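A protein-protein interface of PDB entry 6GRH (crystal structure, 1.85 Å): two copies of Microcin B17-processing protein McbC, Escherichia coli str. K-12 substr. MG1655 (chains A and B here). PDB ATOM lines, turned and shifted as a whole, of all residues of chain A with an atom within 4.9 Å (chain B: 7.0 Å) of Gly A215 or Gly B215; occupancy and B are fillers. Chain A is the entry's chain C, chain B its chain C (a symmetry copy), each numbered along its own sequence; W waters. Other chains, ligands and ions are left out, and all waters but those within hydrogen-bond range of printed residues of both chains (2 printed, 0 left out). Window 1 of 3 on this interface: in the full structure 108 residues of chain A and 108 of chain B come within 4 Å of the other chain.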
ATOM      1  N   LEU A 211     -13.131  10.242  21.542  1.00  0.00           N
ATOM      2  CA  LEU A 211     -12.799  10.985  22.768  1.00  0.00           C
ATOM      3  C   LEU A 211     -12.473  10.045  23.924  1.00  0.00           C
ATOM      4  O   LEU A 211     -11.510  10.250  24.611  1.00  0.00           O
ATOM      5  CB  LEU A 211     -13.915  11.981  23.143  1.00  0.00           C
ATOM      6  CG  LEU A 211     -13.746  13.371  22.526  1.00  0.00           C
ATOM      7  CD1 LEU A 211     -13.570  13.385  21.021  1.00  0.00           C
ATOM      8  CD2 LEU A 211     -14.944  14.239  22.868  1.00  0.00           C
ATOM      9  N   MET A 212     -13.250   8.975  24.078  1.00  0.00           N
ATOM     10  CA  MET A 212     -12.943   7.958  25.062  1.00  0.00           C
ATOM     11  C   MET A 212     -11.598   7.288  24.795  1.00  0.00           C
ATOM     12  O   MET A 212     -10.799   7.100  25.709  1.00  0.00           O
ATOM     13  CB  MET A 212     -14.098   6.946  25.192  1.00  0.00           C
ATOM     14  CG  MET A 212     -15.328   7.600  25.794  1.00  0.00           C
ATOM     15  SD  MET A 212     -16.705   6.475  26.058  1.00  0.00           S
ATOM     16  CE  MET A 212     -17.068   5.911  24.416  1.00  0.00           C
ATOM     17  N   GLU A 213     -11.320   6.990  23.541  1.00  0.00           N
ATOM     18  CA  GLU A 213     -10.058   6.403  23.177  1.00  0.00           C
ATOM     19  C   GLU A 213      -8.870   7.257  23.571  1.00  0.00           C
ATOM     20  O   GLU A 213      -7.885   6.744  24.048  1.00  0.00           O
ATOM     21  CB  GLU A 213     -10.030   6.103  21.693  1.00  0.00           C
ATOM     22  CG  GLU A 213      -8.727   5.546  21.183  1.00  0.00           C
ATOM     23  CD  GLU A 213      -8.824   5.189  19.714  1.00  0.00           C
ATOM     24  OE1 GLU A 213      -9.895   4.631  19.315  1.00  0.00           O
ATOM     25  OE2 GLU A 213      -7.833   5.474  18.972  1.00  0.00           O
ATOM     26  N   THR A 214      -8.990   8.554  23.406  1.00  0.00           N
ATOM     27  CA  THR A 214      -7.955   9.501  23.826  1.00  0.00           C
ATOM     28  C   THR A 214      -7.601   9.371  25.309  1.00  0.00           C
ATOM     29  O   THR A 214      -6.436   9.375  25.670  1.00  0.00           O
ATOM     30  CB  THR A 214      -8.412  10.925  23.492  1.00  0.00           C
ATOM     31  OG1 THR A 214      -8.709  10.974  22.084  1.00  0.00           O
ATOM     32  CG2 THR A 214      -7.352  11.932  23.828  1.00  0.00           C
ATOM     33  N   GLY A 215      -8.634   9.198  26.144  1.00  0.00           N
ATOM     34  CA  GLY A 215      -8.461   8.997  27.556  1.00  0.00           C
ATOM     35  C   GLY A 215      -7.784   7.680  27.870  1.00  0.00           C
ATOM     36  O   GLY A 215      -6.937   7.633  28.780  1.00  0.00           O
ATOM     37  N   SER A 216      -8.121   6.603  27.124  1.00  0.00           N
ATOM     38  CA  SER A 216      -7.405   5.346  27.316  1.00  0.00           C
ATOM     39  C   SER A 216      -5.916   5.503  26.980  1.00  0.00           C
ATOM     40  O   SER A 216      -5.030   4.850  27.597  1.00  0.00           O
ATOM     41  CB  SER A 216      -8.037   4.180  26.516  1.00  0.00           C
ATOM     42  OG  SER A 216      -7.817   4.329  25.132  1.00  0.00           O
ATOM     43  N   MET A 217      -5.626   6.341  26.001  1.00  0.00           N
ATOM     44  CA  MET A 217      -4.245   6.547  25.575  1.00  0.00           C
ATOM     45  C   MET A 217      -3.460   7.346  26.598  1.00  0.00           C
ATOM     46  O   MET A 217      -2.388   6.909  27.018  1.00  0.00           O
ATOM     47  CB  MET A 217      -4.164   7.182  24.201  1.00  0.00           C
ATOM     48  CG  MET A 217      -4.750   6.280  23.140  1.00  0.00           C
ATOM     49  SD  MET A 217      -5.028   7.143  21.598  1.00  0.00           S
ATOM     50  CE  MET A 217      -3.340   7.458  21.102  1.00  0.00           C
ATOM     51  N   TYR A 218      -3.965   8.500  27.028  1.00  0.00           N
ATOM     52  CA  TYR A 218      -3.190   9.265  28.000  1.00  0.00           C
ATOM     53  C   TYR A 218      -3.072   8.533  29.345  1.00  0.00           C
ATOM     54  O   TYR A 218      -2.100   8.742  30.075  1.00  0.00           O
ATOM     55  CB  TYR A 218      -3.648  10.718  28.142  1.00  0.00           C
ATOM     56  CG  TYR A 218      -4.966  11.020  28.832  1.00  0.00           C
ATOM     57  CD1 TYR A 218      -5.212  10.653  30.146  1.00  0.00           C
ATOM     58  CD2 TYR A 218      -5.939  11.779  28.176  1.00  0.00           C
ATOM     59  CE1 TYR A 218      -6.420  10.980  30.762  1.00  0.00           C
ATOM     60  CE2 TYR A 218      -7.144  12.123  28.787  1.00  0.00           C
ATOM     61  CZ  TYR A 218      -7.377  11.733  30.078  1.00  0.00           C
ATOM     62  OH  TYR A 218      -8.577  12.051  30.674  1.00  0.00           O
ATOM     63  N   GLN A 219      -4.038   7.671  29.655  1.00  0.00           N
ATOM     64  CA  GLN A 219      -3.997   6.911  30.896  1.00  0.00           C
ATOM     65  C   GLN A 219      -2.853   5.898  30.885  1.00  0.00           C
ATOM     66  O   GLN A 219      -2.149   5.764  31.873  1.00  0.00           O
ATOM     67  CB  GLN A 219      -5.334   6.210  31.164  1.00  0.00           C
ATOM     68  CG  GLN A 219      -5.425   5.493  32.512  1.00  0.00           C
ATOM     69  CD  GLN A 219      -5.210   6.384  33.739  1.00  0.00           C
ATOM     70  OE1 GLN A 219      -5.307   7.622  33.670  1.00  0.00           O
ATOM     71  NE2 GLN A 219      -4.903   5.741  34.889  1.00  0.00           N
ATOM     72  N   ILE B 129     -17.863  11.238  36.000  1.00  0.00           N
ATOM     73  CA  ILE B 129     -18.268   9.972  35.445  1.00  0.00           C
ATOM     74  C   ILE B 129     -18.546   9.032  36.590  1.00  0.00           C
ATOM     75  O   ILE B 129     -17.731   8.891  37.487  1.00  0.00           O
ATOM     76  CB  ILE B 129     -17.172   9.377  34.524  1.00  0.00           C
ATOM     77  CG1 ILE B 129     -16.846  10.342  33.410  1.00  0.00           C
ATOM     78  CG2 ILE B 129     -17.567   7.998  33.985  1.00  0.00           C
ATOM     79  CD1 ILE B 129     -18.033  10.783  32.581  1.00  0.00           C
ATOM     80  N   TYR B 191     -20.410   3.057  32.364  1.00  0.00           N
ATOM     81  CA  TYR B 191     -19.816   4.339  32.703  1.00  0.00           C
ATOM     82  C   TYR B 191     -20.769   5.426  32.244  1.00  0.00           C
ATOM     83  O   TYR B 191     -21.117   5.463  31.062  1.00  0.00           O
ATOM     84  CB  TYR B 191     -18.450   4.509  32.020  1.00  0.00           C
ATOM     85  CG  TYR B 191     -17.462   3.457  32.373  1.00  0.00           C
ATOM     86  CD1 TYR B 191     -16.518   3.673  33.382  1.00  0.00           C
ATOM     87  CD2 TYR B 191     -17.465   2.205  31.715  1.00  0.00           C
ATOM     88  CE1 TYR B 191     -15.609   2.673  33.732  1.00  0.00           C
ATOM     89  CE2 TYR B 191     -16.542   1.205  32.037  1.00  0.00           C
ATOM     90  CZ  TYR B 191     -15.617   1.446  33.048  1.00  0.00           C
ATOM     91  OH  TYR B 191     -14.690   0.503  33.375  1.00  0.00           O
ATOM     92  N   ALA B 210     -14.971  15.036  30.122  1.00  0.00           N
ATOM     93  CA  ALA B 210     -15.718  13.915  30.713  1.00  0.00           C
ATOM     94  C   ALA B 210     -15.630  12.614  29.881  1.00  0.00           C
ATOM     95  O   ALA B 210     -15.455  11.526  30.441  1.00  0.00           O
ATOM     96  CB  ALA B 210     -17.160  14.303  30.911  1.00  0.00           C
ATOM     97  N   LEU B 211     -15.721  12.749  28.558  1.00  0.00           N
ATOM     98  CA  LEU B 211     -15.604  11.603  27.641  1.00  0.00           C
ATOM     99  C   LEU B 211     -14.206  10.996  27.674  1.00  0.00           C
ATOM    100  O   LEU B 211     -14.070   9.805  27.745  1.00  0.00           O
ATOM    101  CB  LEU B 211     -16.024  11.985  26.206  1.00  0.00           C
ATOM    102  CG  LEU B 211     -17.512  11.779  25.915  1.00  0.00           C
ATOM    103  CD1 LEU B 211     -18.455  12.453  26.891  1.00  0.00           C
ATOM    104  CD2 LEU B 211     -17.841  12.281  24.520  1.00  0.00           C
ATOM    105  N   MET B 212     -13.175  11.839  27.695  1.00  0.00           N
ATOM    106  CA  MET B 212     -11.818  11.362  27.859  1.00  0.00           C
ATOM    107  C   MET B 212     -11.618  10.646  29.192  1.00  0.00           C
ATOM    108  O   MET B 212     -11.015   9.577  29.244  1.00  0.00           O
ATOM    109  CB  MET B 212     -10.800  12.498  27.633  1.00  0.00           C
ATOM    110  CG  MET B 212     -10.800  12.947  26.184  1.00  0.00           C
ATOM    111  SD  MET B 212      -9.586  14.218  25.808  1.00  0.00           S
ATOM    112  CE  MET B 212     -10.090  15.561  26.852  1.00  0.00           C
ATOM    113  N   GLU B 213     -12.175  11.195  30.253  1.00  0.00           N
ATOM    114  CA  GLU B 213     -12.089  10.572  31.546  1.00  0.00           C
ATOM    115  C   GLU B 213     -12.669   9.172  31.572  1.00  0.00           C
ATOM    116  O   GLU B 213     -12.098   8.289  32.167  1.00  0.00           O
ATOM    117  CB  GLU B 213     -12.754  11.443  32.591  1.00  0.00           C
ATOM    118  CG  GLU B 213     -12.784  10.858  33.979  1.00  0.00           C
ATOM    119  CD  GLU B 213     -13.380  11.837  34.970  1.00  0.00           C
ATOM    120  OE1 GLU B 213     -13.051  13.060  34.858  1.00  0.00           O
ATOM    121  OE2 GLU B 213     -14.175  11.376  35.848  1.00  0.00           O
ATOM    122  N   THR B 214     -13.774   8.975  30.892  1.00  0.00           N
ATOM    123  CA  THR B 214     -14.393   7.655  30.759  1.00  0.00           C
ATOM    124  C   THR B 214     -13.437   6.610  30.179  1.00  0.00           C
ATOM    125  O   THR B 214     -13.365   5.496  30.671  1.00  0.00           O
ATOM    126  CB  THR B 214     -15.659   7.777  29.905  1.00  0.00           C
ATOM    127  OG1 THR B 214     -16.512   8.759  30.520  1.00  0.00           O
ATOM    128  CG2 THR B 214     -16.378   6.465  29.803  1.00  0.00           C
ATOM    129  N   GLY B 215     -12.670   7.020  29.162  1.00  0.00           N
ATOM    130  CA  GLY B 215     -11.678   6.176  28.552  1.00  0.00           C
ATOM    131  C   GLY B 215     -10.535   5.861  29.493  1.00  0.00           C
ATOM    132  O   GLY B 215     -10.052   4.715  29.500  1.00  0.00           O
ATOM    133  N   SER B 216     -10.098   6.847  30.309  1.00  0.00           N
ATOM    134  CA  SER B 216      -9.080   6.549  31.311  1.00  0.00           C
ATOM    135  C   SER B 216      -9.590   5.514  32.323  1.00  0.00           C
ATOM    136  O   SER B 216      -8.813   4.674  32.853  1.00  0.00           O
ATOM    137  CB  SER B 216      -8.570   7.824  32.028  1.00  0.00           C
ATOM    138  OG  SER B 216      -9.551   8.358  32.888  1.00  0.00           O
ATOM    139  N   MET B 217     -10.878   5.570  32.614  1.00  0.00           N
ATOM    140  CA  MET B 217     -11.467   4.654  33.586  1.00  0.00           C
ATOM    141  C   MET B 217     -11.574   3.247  33.031  1.00  0.00           C
ATOM    142  O   MET B 217     -11.108   2.304  33.671  1.00  0.00           O
ATOM    143  CB  MET B 217     -12.808   5.150  34.091  1.00  0.00           C
ATOM    144  CG  MET B 217     -12.667   6.452  34.845  1.00  0.00           C
ATOM    145  SD  MET B 217     -14.244   7.254  35.107  1.00  0.00           S
ATOM    146  CE  MET B 217     -15.000   6.102  36.247  1.00  0.00           C
ATOM    147  N   TYR B 218     -12.159   3.072  31.848  1.00  0.00           N
ATOM    148  CA  TYR B 218     -12.269   1.710  31.336  1.00  0.00           C
ATOM    149  C   TYR B 218     -10.894   1.102  31.020  1.00  0.00           C
ATOM    150  O   TYR B 218     -10.736  -0.120  31.068  1.00  0.00           O
ATOM    151  CB  TYR B 218     -13.270   1.566  30.187  1.00  0.00           C
ATOM    152  CG  TYR B 218     -12.928   2.140  28.824  1.00  0.00           C
ATOM    153  CD1 TYR B 218     -11.815   1.728  28.108  1.00  0.00           C
ATOM    154  CD2 TYR B 218     -13.802   3.038  28.206  1.00  0.00           C
ATOM    155  CE1 TYR B 218     -11.551   2.248  26.842  1.00  0.00           C
ATOM    156  CE2 TYR B 218     -13.556   3.553  26.935  1.00  0.00           C
ATOM    157  CZ  TYR B 218     -12.439   3.151  26.253  1.00  0.00           C
ATOM    158  OH  TYR B 218     -12.182   3.678  25.007  1.00  0.00           O
ATOM    159  N   GLN B 219      -9.909   1.948  30.723  1.00  0.00           N
ATOM    160  CA  GLN B 219      -8.566   1.466  30.436  1.00  0.00           C
ATOM    161  C   GLN B 219      -7.916   0.869  31.685  1.00  0.00           C
ATOM    162  O   GLN B 219      -7.300  -0.181  31.606  1.00  0.00           O
ATOM    163  CB  GLN B 219      -7.688   2.578  29.852  1.00  0.00           C
ATOM    164  CG  GLN B 219      -6.297   2.129  29.400  1.00  0.00           C
ATOM    165  CD  GLN B 219      -6.282   1.032  28.331  1.00  0.00           C
ATOM    166  OE1 GLN B 219      -7.287   0.782  27.641  1.00  0.00           O
ATOM    167  NE2 GLN B 219      -5.119   0.356  28.195  1.00  0.00           N
ATOM    168  N   ASN B 220      -8.067   1.527  32.826  1.00  0.00           N
ATOM    169  CA  ASN B 220      -7.657   0.944  34.113  1.00  0.00           C
ATOM    170  C   ASN B 220      -8.317  -0.413  34.353  1.00  0.00           C
ATOM    171  O   ASN B 220      -7.676  -1.350  34.863  1.00  0.00           O
ATOM    172  CB  ASN B 220      -7.997   1.869  35.289  1.00  0.00           C
ATOM    173  CG  ASN B 220      -6.900   2.849  35.599  1.00  0.00           C
ATOM    174  OD1 ASN B 220      -5.955   2.990  34.832  1.00  0.00           O
ATOM    175  ND2 ASN B 220      -7.033   3.556  36.736  1.00  0.00           N
ATOM    176  N   ALA B 221      -9.593  -0.495  34.012  1.00  0.00           N
ATOM    177  CA  ALA B 221     -10.343  -1.735  34.135  1.00  0.00           C
ATOM    178  C   ALA B 221      -9.831  -2.835  33.190  1.00  0.00           C
ATOM    179  O   ALA B 221      -9.728  -3.973  33.604  1.00  0.00           O
ATOM    180  CB  ALA B 221     -11.826  -1.493  33.953  1.00  0.00           C
ATOM    181  N   ILE B 258     -20.648   4.202  27.761  1.00  0.00           N
ATOM    182  CA  ILE B 258     -19.998   2.995  27.282  1.00  0.00           C
ATOM    183  C   ILE B 258     -20.264   1.881  28.285  1.00  0.00           C
ATOM    184  O   ILE B 258     -20.438   2.126  29.492  1.00  0.00           O
ATOM    185  CB  ILE B 258     -18.487   3.242  27.023  1.00  0.00           C
ATOM    186  CG1 ILE B 258     -17.882   2.212  26.092  1.00  0.00           C
ATOM    187  CG2 ILE B 258     -17.689   3.330  28.309  1.00  0.00           C
ATOM    188  CD1 ILE B 258     -18.366   2.327  24.666  1.00  0.00           C
HETATM  189  O   HOH W   1      -9.790   2.966  24.028  1.00  0.00           O
HETATM  190  O   HOH W   2      -8.903  10.910  33.077  1.00  0.00           O
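Of chain B, only Met B212, Gly B215 and Ser B216 come within 4 Å of Gly A215.
Printed residues of chain B within 4 Å of Leu A211: Leu B211 and Met B212.
Of the printed residues of chain A, Asn B220 touches Gln A219 (2.9 Å).
Printed residues of chain B within 4 Å of Glu A213: Tyr B218.
Printed residues of chain A within 4 Å of Leu B211: Leu A211 and Met A212.
Ala B221 touches none of the printed residues of chain A.
The nearest printed residue of chain A that does not touch Gly B215 is Glu A213 (5.1 Å).
The nearest printed residue of chain B that does not touch Leu A211 is Gly B215 (5.7 Å).
Water W1 bridges the side-chain hydroxyl (OG) of Ser A216 and the side-chain hydroxyl (OH) of Tyr B218.
Water W2 lies within hydrogen-bond range of OG of Ser B216 (2.6 Å) and OH of Tyr A218 (2.7 Å).
O of Ile B258 lies within hydrogen-bond range of N of Tyr B191 (3.0 Å).
The backbone carbonyl oxygen (O) of Glu A213 is in hydrogen-bond range of the side-chain hydroxyl (OG) of Ser A216, 2.6 Å away.
The backbone carbonyl oxygen (O) of Ala B210 sits at hydrogen-bond distance from the side-chain hydroxyl (OG1) of Thr B214, 3.0 Å away.
The backbone carbonyl oxygen (O) of Glu B213 is in hydrogen-bond range of the side-chain hydroxyl (OG) of Ser B216, at 2.6 Å.
NE2 of Gln A219 lies within hydrogen-bond range of OD1 of Asn B220, at 2.9 Å.
Leu B211 touches its own counterpart, Leu A211.
Met A212 touches Thr B214, and with the chains exchanged Thr A214 touches Met B212.
Gly B215 touches its own counterpart, Gly A215.
Gly A215 touches Ser B216, and with the chains exchanged Ser A216 touches Gly B215.
Among the printed residues, merely in contact across the chains: Gly A215 with Met B212, Met A212 with Gly B215, Met A212 with Leu B211, Leu A211 with Met B212, Ser A216 with Gly B215, Gly A215 with Ser B216, Ser A216 with Gln B219, Gln A219 with Ser B216, Tyr A218 with Met B212, Met A212 with Tyr B218, Gly A215 with Gly B215, Leu A211 with Leu B211, Tyr A218 with Glu B213, Glu A213 with Tyr B218, Ser A216 with Ser B216, Met A212 with Thr B214, Thr A214 with Met B212 and Met A212 with Ile B258.
Of the 9 printed residues of chain A, 8 touch a printed residue of chain B.
Hydrophobic or aromatic side chains of chain B within 4 Å of the printed part of chain A: Leu B211, Met B212, Tyr B218 and Ile B258.
Among the printed residues, 19 pairs touch across the chains.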
